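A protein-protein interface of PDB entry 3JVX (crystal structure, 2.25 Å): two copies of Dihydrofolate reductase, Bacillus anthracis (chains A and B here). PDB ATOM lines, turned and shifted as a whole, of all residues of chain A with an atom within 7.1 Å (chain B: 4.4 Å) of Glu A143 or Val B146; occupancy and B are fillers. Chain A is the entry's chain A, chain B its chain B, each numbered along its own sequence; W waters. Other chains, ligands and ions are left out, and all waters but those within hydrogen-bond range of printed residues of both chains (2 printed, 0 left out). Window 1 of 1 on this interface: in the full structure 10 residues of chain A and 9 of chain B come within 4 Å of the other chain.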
ATOM      1  N   LYS A 122      12.351  16.889  33.778  1.00  0.00           N
ATOM      2  CA  LYS A 122      12.704  18.058  34.569  1.00  0.00           C
ATOM      3  C   LYS A 122      12.341  17.844  36.034  1.00  0.00           C
ATOM      4  O   LYS A 122      11.175  17.673  36.378  1.00  0.00           O
ATOM      5  CB  LYS A 122      12.040  19.322  34.002  1.00  0.00           C
ATOM      6  CG  LYS A 122      12.509  19.656  32.578  1.00  0.00           C
ATOM      7  CD  LYS A 122      11.706  20.795  31.975  1.00  0.00           C
ATOM      8  CE  LYS A 122      12.253  21.185  30.608  1.00  0.00           C
ATOM      9  NZ  LYS A 122      11.477  22.339  30.054  1.00  0.00           N
ATOM     10  N   MET A 138      15.389  26.868  22.202  1.00  0.00           N
ATOM     11  CA  MET A 138      14.229  26.040  21.863  1.00  0.00           C
ATOM     12  C   MET A 138      13.352  26.648  20.776  1.00  0.00           C
ATOM     13  O   MET A 138      12.272  26.131  20.488  1.00  0.00           O
ATOM     14  CB  MET A 138      13.407  25.693  23.110  1.00  0.00           C
ATOM     15  CG  MET A 138      14.142  24.799  24.116  1.00  0.00           C
ATOM     16  SD  MET A 138      14.871  23.331  23.356  1.00  0.00           S
ATOM     17  CE  MET A 138      13.428  22.302  23.121  1.00  0.00           C
ATOM     18  N   TRP A 141      11.412  24.562  18.140  1.00  0.00           N
ATOM     19  CA  TRP A 141      11.077  23.295  18.769  1.00  0.00           C
ATOM     20  C   TRP A 141       9.674  23.385  19.318  1.00  0.00           C
ATOM     21  O   TRP A 141       9.224  24.458  19.728  1.00  0.00           O
ATOM     22  CB  TRP A 141      12.045  22.979  19.893  1.00  0.00           C
ATOM     23  CG  TRP A 141      13.389  22.576  19.420  1.00  0.00           C
ATOM     24  CD1 TRP A 141      14.332  23.375  18.843  1.00  0.00           C
ATOM     25  CD2 TRP A 141      13.958  21.268  19.496  1.00  0.00           C
ATOM     26  NE1 TRP A 141      15.459  22.644  18.549  1.00  0.00           N
ATOM     27  CE2 TRP A 141      15.257  21.344  18.939  1.00  0.00           C
ATOM     28  CE3 TRP A 141      13.496  20.036  19.972  1.00  0.00           C
ATOM     29  CZ2 TRP A 141      16.102  20.233  18.853  1.00  0.00           C
ATOM     30  CZ3 TRP A 141      14.334  18.934  19.888  1.00  0.00           C
ATOM     31  CH2 TRP A 141      15.626  19.043  19.338  1.00  0.00           C
ATOM     32  N   LYS A 142       8.971  22.260  19.311  1.00  0.00           N
ATOM     33  CA  LYS A 142       7.633  22.197  19.886  1.00  0.00           C
ATOM     34  C   LYS A 142       7.543  21.076  20.898  1.00  0.00           C
ATOM     35  O   LYS A 142       8.027  19.972  20.648  1.00  0.00           O
ATOM     36  CB  LYS A 142       6.571  22.016  18.799  1.00  0.00           C
ATOM     37  CG  LYS A 142       6.323  23.292  18.017  1.00  0.00           C
ATOM     38  CD  LYS A 142       5.172  23.164  17.048  1.00  0.00           C
ATOM     39  CE  LYS A 142       5.033  24.446  16.265  1.00  0.00           C
ATOM     40  NZ  LYS A 142       4.085  24.273  15.150  1.00  0.00           N
ATOM     41  N   GLU A 143       6.926  21.364  22.042  1.00  0.00           N
ATOM     42  CA  GLU A 143       6.618  20.325  23.020  1.00  0.00           C
ATOM     43  C   GLU A 143       5.498  19.450  22.460  1.00  0.00           C
ATOM     44  O   GLU A 143       4.429  19.952  22.103  1.00  0.00           O
ATOM     45  CB  GLU A 143       6.196  20.930  24.367  1.00  0.00           C
ATOM     46  CG  GLU A 143       6.112  19.913  25.507  1.00  0.00           C
ATOM     47  CD  GLU A 143       5.744  20.536  26.841  1.00  0.00           C
ATOM     48  OE1 GLU A 143       6.624  20.578  27.716  1.00  0.00           O
ATOM     49  OE2 GLU A 143       4.586  20.990  27.022  1.00  0.00           O
ATOM     50  N   VAL A 144       5.758  18.148  22.360  1.00  0.00           N
ATOM     51  CA  VAL A 144       4.778  17.203  21.806  1.00  0.00           C
ATOM     52  C   VAL A 144       4.276  16.203  22.849  1.00  0.00           C
ATOM     53  O   VAL A 144       3.379  15.406  22.578  1.00  0.00           O
ATOM     54  CB  VAL A 144       5.322  16.418  20.584  1.00  0.00           C
ATOM     55  CG1 VAL A 144       5.760  17.367  19.479  1.00  0.00           C
ATOM     56  CG2 VAL A 144       6.456  15.494  20.992  1.00  0.00           C
ATOM     57  N   PHE A 145       4.869  16.240  24.037  1.00  0.00           N
ATOM     58  CA  PHE A 145       4.449  15.388  25.140  1.00  0.00           C
ATOM     59  C   PHE A 145       4.886  15.987  26.467  1.00  0.00           C
ATOM     60  O   PHE A 145       6.018  16.444  26.612  1.00  0.00           O
ATOM     61  CB  PHE A 145       5.011  13.953  25.008  1.00  0.00           C
ATOM     62  CG  PHE A 145       4.581  13.029  26.128  1.00  0.00           C
ATOM     63  CD1 PHE A 145       3.306  12.449  26.121  1.00  0.00           C
ATOM     64  CD2 PHE A 145       5.441  12.750  27.199  1.00  0.00           C
ATOM     65  CE1 PHE A 145       2.897  11.606  27.152  1.00  0.00           C
ATOM     66  CE2 PHE A 145       5.032  11.911  28.254  1.00  0.00           C
ATOM     67  CZ  PHE A 145       3.763  11.336  28.223  1.00  0.00           C
ATOM     68  N   VAL A 146       3.976  15.970  27.432  1.00  0.00           N
ATOM     69  CA  VAL A 146       4.301  16.328  28.811  1.00  0.00           C
ATOM     70  C   VAL A 146       3.416  15.540  29.793  1.00  0.00           C
ATOM     71  O   VAL A 146       2.218  15.328  29.552  1.00  0.00           O
ATOM     72  CB  VAL A 146       4.269  17.877  29.060  1.00  0.00           C
ATOM     73  CG1 VAL A 146       2.889  18.455  28.768  1.00  0.00           C
ATOM     74  CG2 VAL A 146       4.736  18.223  30.471  1.00  0.00           C
ATOM     75  N   GLU A 147       4.025  15.082  30.884  1.00  0.00           N
ATOM     76  CA  GLU A 147       3.310  14.303  31.894  1.00  0.00           C
ATOM     77  C   GLU A 147       4.032  14.371  33.235  1.00  0.00           C
ATOM     78  O   GLU A 147       5.257  14.314  33.286  1.00  0.00           O
ATOM     79  CB  GLU A 147       3.156  12.844  31.442  1.00  0.00           C
ATOM     80  CG  GLU A 147       2.105  12.037  32.214  1.00  0.00           C
ATOM     81  CD  GLU A 147       1.910  10.650  31.638  1.00  0.00           C
ATOM     82  OE1 GLU A 147       1.260  10.540  30.575  1.00  0.00           O
ATOM     83  OE2 GLU A 147       2.403   9.667  32.234  1.00  0.00           O
ATOM     84  N   TYR A 161       8.022  14.567  32.784  1.00  0.00           N
ATOM     85  CA  TYR A 161       8.537  14.113  31.502  1.00  0.00           C
ATOM     86  C   TYR A 161       8.146  15.117  30.430  1.00  0.00           C
ATOM     87  O   TYR A 161       6.975  15.506  30.339  1.00  0.00           O
ATOM     88  CB  TYR A 161       7.956  12.734  31.159  1.00  0.00           C
ATOM     89  CG  TYR A 161       8.243  11.669  32.195  1.00  0.00           C
ATOM     90  CD1 TYR A 161       7.213  11.078  32.910  1.00  0.00           C
ATOM     91  CD2 TYR A 161       9.557  11.263  32.465  1.00  0.00           C
ATOM     92  CE1 TYR A 161       7.475  10.094  33.870  1.00  0.00           C
ATOM     93  CE2 TYR A 161       9.826  10.293  33.420  1.00  0.00           C
ATOM     94  CZ  TYR A 161       8.780   9.709  34.114  1.00  0.00           C
ATOM     95  OH  TYR A 161       9.035   8.741  35.054  1.00  0.00           O
ATOM     96  N   HIS A 162       9.119  15.543  29.635  1.00  0.00           N
ATOM     97  CA  HIS A 162       8.874  16.425  28.486  1.00  0.00           C
ATOM     98  C   HIS A 162       9.472  15.819  27.231  1.00  0.00           C
ATOM     99  O   HIS A 162      10.551  15.235  27.277  1.00  0.00           O
ATOM    100  CB  HIS A 162       9.516  17.801  28.689  1.00  0.00           C
ATOM    101  CG  HIS A 162       9.061  18.516  29.921  1.00  0.00           C
ATOM    102  ND1 HIS A 162       8.112  19.513  29.895  1.00  0.00           N
ATOM    103  CD2 HIS A 162       9.440  18.392  31.214  1.00  0.00           C
ATOM    104  CE1 HIS A 162       7.904  19.955  31.123  1.00  0.00           C
ATOM    105  NE2 HIS A 162       8.711  19.304  31.939  1.00  0.00           N
ATOM    106  N   VAL A 163       8.771  15.974  26.113  1.00  0.00           N
ATOM    107  CA  VAL A 163       9.321  15.638  24.803  1.00  0.00           C
ATOM    108  C   VAL A 163       9.165  16.827  23.852  1.00  0.00           C
ATOM    109  O   VAL A 163       8.061  17.340  23.656  1.00  0.00           O
ATOM    110  CB  VAL A 163       8.687  14.356  24.204  1.00  0.00           C
ATOM    111  CG1 VAL A 163       9.398  13.944  22.903  1.00  0.00           C
ATOM    112  CG2 VAL A 163       8.731  13.202  25.221  1.00  0.00           C
ATOM    113  N   TYR A 164      10.282  17.273  23.290  1.00  0.00           N
ATOM    114  CA  TYR A 164      10.276  18.320  22.281  1.00  0.00           C
ATOM    115  C   TYR A 164      10.766  17.774  20.940  1.00  0.00           C
ATOM    116  O   TYR A 164      11.668  16.950  20.906  1.00  0.00           O
ATOM    117  CB  TYR A 164      11.172  19.482  22.708  1.00  0.00           C
ATOM    118  CG  TYR A 164      10.826  20.116  24.037  1.00  0.00           C
ATOM    119  CD1 TYR A 164      10.029  21.266  24.099  1.00  0.00           C
ATOM    120  CD2 TYR A 164      11.318  19.591  25.230  1.00  0.00           C
ATOM    121  CE1 TYR A 164       9.721  21.863  25.316  1.00  0.00           C
ATOM    122  CE2 TYR A 164      11.010  20.178  26.458  1.00  0.00           C
ATOM    123  CZ  TYR A 164      10.218  21.315  26.491  1.00  0.00           C
ATOM    124  OH  TYR A 164       9.929  21.898  27.706  1.00  0.00           O
ATOM    125  N   GLU A 165      10.167  18.241  19.851  1.00  0.00           N
ATOM    126  CA  GLU A 165      10.591  17.887  18.495  1.00  0.00           C
ATOM    127  C   GLU A 165      11.030  19.130  17.730  1.00  0.00           C
ATOM    128  O   GLU A 165      10.346  20.147  17.761  1.00  0.00           O
ATOM    129  CB  GLU A 165       9.457  17.196  17.729  1.00  0.00           C
ATOM    130  CG  GLU A 165       9.041  15.852  18.286  1.00  0.00           C
ATOM    131  CD  GLU A 165       8.070  15.085  17.377  1.00  0.00           C
ATOM    132  OE1 GLU A 165       7.469  15.679  16.448  1.00  0.00           O
ATOM    133  OE2 GLU A 165       7.914  13.869  17.600  1.00  0.00           O
ATOM    134  N   GLN A 167      11.399  21.492  14.669  1.00  0.00           N
ATOM    135  CA  GLN A 167      10.562  21.737  13.503  1.00  0.00           C
ATOM    136  C   GLN A 167      11.398  21.833  12.222  1.00  0.00           C
ATOM    137  O   GLN A 167      11.032  21.250  11.203  1.00  0.00           O
ATOM    138  CB  GLN A 167       9.637  22.940  13.722  1.00  0.00           C
ATOM    139  CG  GLN A 167       8.711  22.788  14.953  1.00  0.00           C
ATOM    140  CD  GLN A 167       7.793  21.567  14.878  1.00  0.00           C
ATOM    141  OE1 GLN A 167       6.861  21.535  14.083  1.00  0.00           O
ATOM    142  NE2 GLN A 167       8.055  20.565  15.713  1.00  0.00           N
ATOM    143  N   GLU B 143       4.237  29.759  14.265  1.00  0.00           N
ATOM    144  CA  GLU B 143       4.540  29.353  15.624  1.00  0.00           C
ATOM    145  C   GLU B 143       5.884  28.630  15.647  1.00  0.00           C
ATOM    146  O   GLU B 143       6.053  27.603  14.984  1.00  0.00           O
ATOM    147  CB  GLU B 143       3.433  28.459  16.180  1.00  0.00           C
ATOM    148  CG  GLU B 143       3.575  28.197  17.673  1.00  0.00           C
ATOM    149  CD  GLU B 143       2.562  27.218  18.181  1.00  0.00           C
ATOM    150  OE1 GLU B 143       1.773  27.585  19.072  1.00  0.00           O
ATOM    151  OE2 GLU B 143       2.545  26.069  17.687  1.00  0.00           O
ATOM    152  N   PHE B 145       7.548  28.025  18.780  1.00  0.00           N
ATOM    153  CA  PHE B 145       7.684  27.385  20.081  1.00  0.00           C
ATOM    154  C   PHE B 145       6.341  27.312  20.776  1.00  0.00           C
ATOM    155  O   PHE B 145       5.553  28.266  20.735  1.00  0.00           O
ATOM    156  CB  PHE B 145       8.690  28.129  20.970  1.00  0.00           C
ATOM    157  CG  PHE B 145       8.917  27.467  22.308  1.00  0.00           C
ATOM    158  CD1 PHE B 145       9.589  26.245  22.391  1.00  0.00           C
ATOM    159  CD2 PHE B 145       8.427  28.046  23.477  1.00  0.00           C
ATOM    160  CE1 PHE B 145       9.790  25.627  23.618  1.00  0.00           C
ATOM    161  CE2 PHE B 145       8.626  27.439  24.709  1.00  0.00           C
ATOM    162  CZ  PHE B 145       9.316  26.229  24.782  1.00  0.00           C
ATOM    163  N   VAL B 146       6.090  26.170  21.405  1.00  0.00           N
ATOM    164  CA  VAL B 146       4.925  25.978  22.270  1.00  0.00           C
ATOM    165  C   VAL B 146       5.286  25.004  23.399  1.00  0.00           C
ATOM    166  O   VAL B 146       6.006  24.025  23.184  1.00  0.00           O
ATOM    167  CB  VAL B 146       3.661  25.527  21.479  1.00  0.00           C
ATOM    168  CG1 VAL B 146       3.872  24.182  20.774  1.00  0.00           C
ATOM    169  CG2 VAL B 146       2.435  25.482  22.394  1.00  0.00           C
ATOM    170  N   GLU B 147       4.801  25.296  24.598  1.00  0.00           N
ATOM    171  CA  GLU B 147       5.069  24.472  25.773  1.00  0.00           C
ATOM    172  C   GLU B 147       3.986  24.723  26.835  1.00  0.00           C
ATOM    173  O   GLU B 147       3.524  25.852  27.002  1.00  0.00           O
ATOM    174  CB  GLU B 147       6.477  24.809  26.273  1.00  0.00           C
ATOM    175  CG  GLU B 147       6.850  24.389  27.662  1.00  0.00           C
ATOM    176  CD  GLU B 147       8.256  24.818  28.003  1.00  0.00           C
ATOM    177  OE1 GLU B 147       9.208  24.167  27.531  1.00  0.00           O
ATOM    178  OE2 GLU B 147       8.416  25.812  28.741  1.00  0.00           O
ATOM    179  N   LYS B 148       3.564  23.658  27.514  1.00  0.00           N
ATOM    180  CA  LYS B 148       2.606  23.751  28.604  1.00  0.00           C
ATOM    181  C   LYS B 148       3.247  24.453  29.800  1.00  0.00           C
ATOM    182  O   LYS B 148       4.380  24.133  30.189  1.00  0.00           O
ATOM    183  CB  LYS B 148       2.115  22.347  28.991  1.00  0.00           C
ATOM    184  CG  LYS B 148       1.011  22.320  30.046  1.00  0.00           C
ATOM    185  CD  LYS B 148       0.296  20.977  30.088  1.00  0.00           C
ATOM    186  CE  LYS B 148      -1.056  21.055  30.805  1.00  0.00           C
ATOM    187  NZ  LYS B 148      -0.909  21.560  32.190  1.00  0.00           N
ATOM    188  N   TYR B 161       2.743  28.532  26.875  1.00  0.00           N
ATOM    189  CA  TYR B 161       3.641  29.536  26.317  1.00  0.00           C
ATOM    190  C   TYR B 161       3.665  29.306  24.822  1.00  0.00           C
ATOM    191  O   TYR B 161       3.822  28.163  24.381  1.00  0.00           O
ATOM    192  CB  TYR B 161       5.062  29.388  26.886  1.00  0.00           C
ATOM    193  CG  TYR B 161       5.149  29.493  28.393  1.00  0.00           C
ATOM    194  CD1 TYR B 161       5.493  28.379  29.182  1.00  0.00           C
ATOM    195  CD2 TYR B 161       4.885  30.709  29.038  1.00  0.00           C
ATOM    196  CE1 TYR B 161       5.584  28.472  30.568  1.00  0.00           C
ATOM    197  CE2 TYR B 161       4.963  30.820  30.430  1.00  0.00           C
ATOM    198  CZ  TYR B 161       5.317  29.701  31.190  1.00  0.00           C
ATOM    199  OH  TYR B 161       5.394  29.842  32.564  1.00  0.00           O
ATOM    200  N   HIS B 162       3.474  30.375  24.052  1.00  0.00           N
ATOM    201  CA  HIS B 162       3.568  30.333  22.592  1.00  0.00           C
ATOM    202  C   HIS B 162       4.510  31.417  22.122  1.00  0.00           C
ATOM    203  O   HIS B 162       4.537  32.509  22.682  1.00  0.00           O
ATOM    204  CB  HIS B 162       2.222  30.583  21.922  1.00  0.00           C
ATOM    205  CG  HIS B 162       1.160  29.603  22.296  1.00  0.00           C
ATOM    206  ND1 HIS B 162       0.782  28.567  21.471  1.00  0.00           N
ATOM    207  CD2 HIS B 162       0.375  29.515  23.397  1.00  0.00           C
ATOM    208  CE1 HIS B 162      -0.186  27.878  22.051  1.00  0.00           C
ATOM    209  NE2 HIS B 162      -0.455  28.435  23.217  1.00  0.00           N
HETATM  210  O   HOH W   1       6.205  22.136  29.917  1.00  0.00           O
HETATM  211  O   HOH W   2       9.179  23.342  30.893  1.00  0.00           O
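The backbone carbonyl oxygen (O) of Val B146 is in hydrogen-bond range of the backbone NH (N) of Glu A143, at 3.0 Å.
OE1 of Glu B147 lies within salt-bridge range of NZ of Lys A122, 3.9 Å away.
The side-chain hydroxyl (OH) of Tyr A164 lies close to the side-chain carboxylate (OE1) of Glu B147.
The side-chain amino group (NZ) of Lys A142 is in salt-bridge range of the side-chain carboxylate (OE2) of Glu B143, at 3.5 Å.
The backbone NH (N) of Lys B148 is in hydrogen-bond range of the side-chain carboxylate (OE2) of Glu A143 (2.9 Å).
The side-chain carboxylate of Glu B143 is in hydrogen-bond range of a ring nitrogen (ND1) of His B162 (2.8 Å).
OE1 of Glu A143 lies within hydrogen-bond range of ND1 of His A162, 2.8 Å away.
The backbone carbonyl oxygen (O) of Glu B147 sits at hydrogen-bond distance from the backbone NH (N) of Tyr B161 (2.8 Å).
The side-chain amino group (NZ) of Lys A122 is in hydrogen-bond range of the side-chain hydroxyl (OH) of Tyr A164 (2.8 Å).
The backbone carbonyl oxygen (O) of Lys A142 is in hydrogen-bond range of the backbone NH (N) of Glu A165, 2.9 Å away.
CD1 of Phe B145 touches O of Met A138, at 3.3 Å.
Trp A141 touches Phe B145 (O to CD1, 3.2 Å).
Trp A141 touches Val B146 (O to N, 3.9 Å).
Val B146 touches Lys A142 (CG1 to CG, 3.8 Å).
Glu A143 touches Glu B147 (OE2 to CA, 3.7 Å).
CG1 of Val A146 touches CD of Lys B148, at 3.9 Å.
Glu A143 touches just these residues of chain B: Val B146 (3.0 Å), Glu B147 (3.7 Å) and Lys B148 (2.9 Å).
Tyr A161 touches none of the printed residues of chain B.
His A162 touches none of the printed residues of chain B.
Of the printed residues of chain A, Glu B143 touches Lys A142.
Val B146 touches just these residues of chain A: Trp A141, Lys A142 and Glu A143.
Of the printed residues of chain A, Lys B148 touches Glu A143 and Val A146.
The nearest residue of chain A that does not touch Val B146 is Tyr A164 (4.8 Å).
Hydrophobic or aromatic side chains of chain B within 4 Å of the printed part of chain A: Phe B145 and Val B146.
Of the 15 printed residues of chain A, 7 touch a printed residue of chain B.
Printed residues of chain A that touch a printed residue of chain B: Lys A122, Met A138, Trp A141, Lys A142, Glu A143, Val A146 and Tyr A164.
Among the printed residues, 11 pairs touch across the chains.
Among the printed residues, Asp or Glu carboxylates within 4 Å of a Lys or Arg side-chain nitrogen of the other chain: Lys A122 with Glu B147 (3.9 Å) and Lys A142 with Glu B143 (3.5 Å).
Glu A143 touches Val B146, but with the chains exchanged Val A146 does not touch Glu B143 (13.4 Å).
Glu A143 touches Glu B147, but with the chains exchanged Glu A147 does not touch Glu B143 (17.2 Å).
6 positions are printed for both chains.
Of the 11 pairs that touch across the chains among the printed residues, none has its exchanged pair printed and touching as well.
Water W2 lies within hydrogen-bond range of the side-chain amino group (NZ) of Lys A122 (2.6 Å) and the side-chain carboxylate (OE2) of Glu B147 (3.4 Å).
Water W1 lies within hydrogen-bond range of O of Lys B148 (2.7 Å), OE1 of Glu A143 (2.7 Å) and ND1 of His A162 (3.2 Å).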
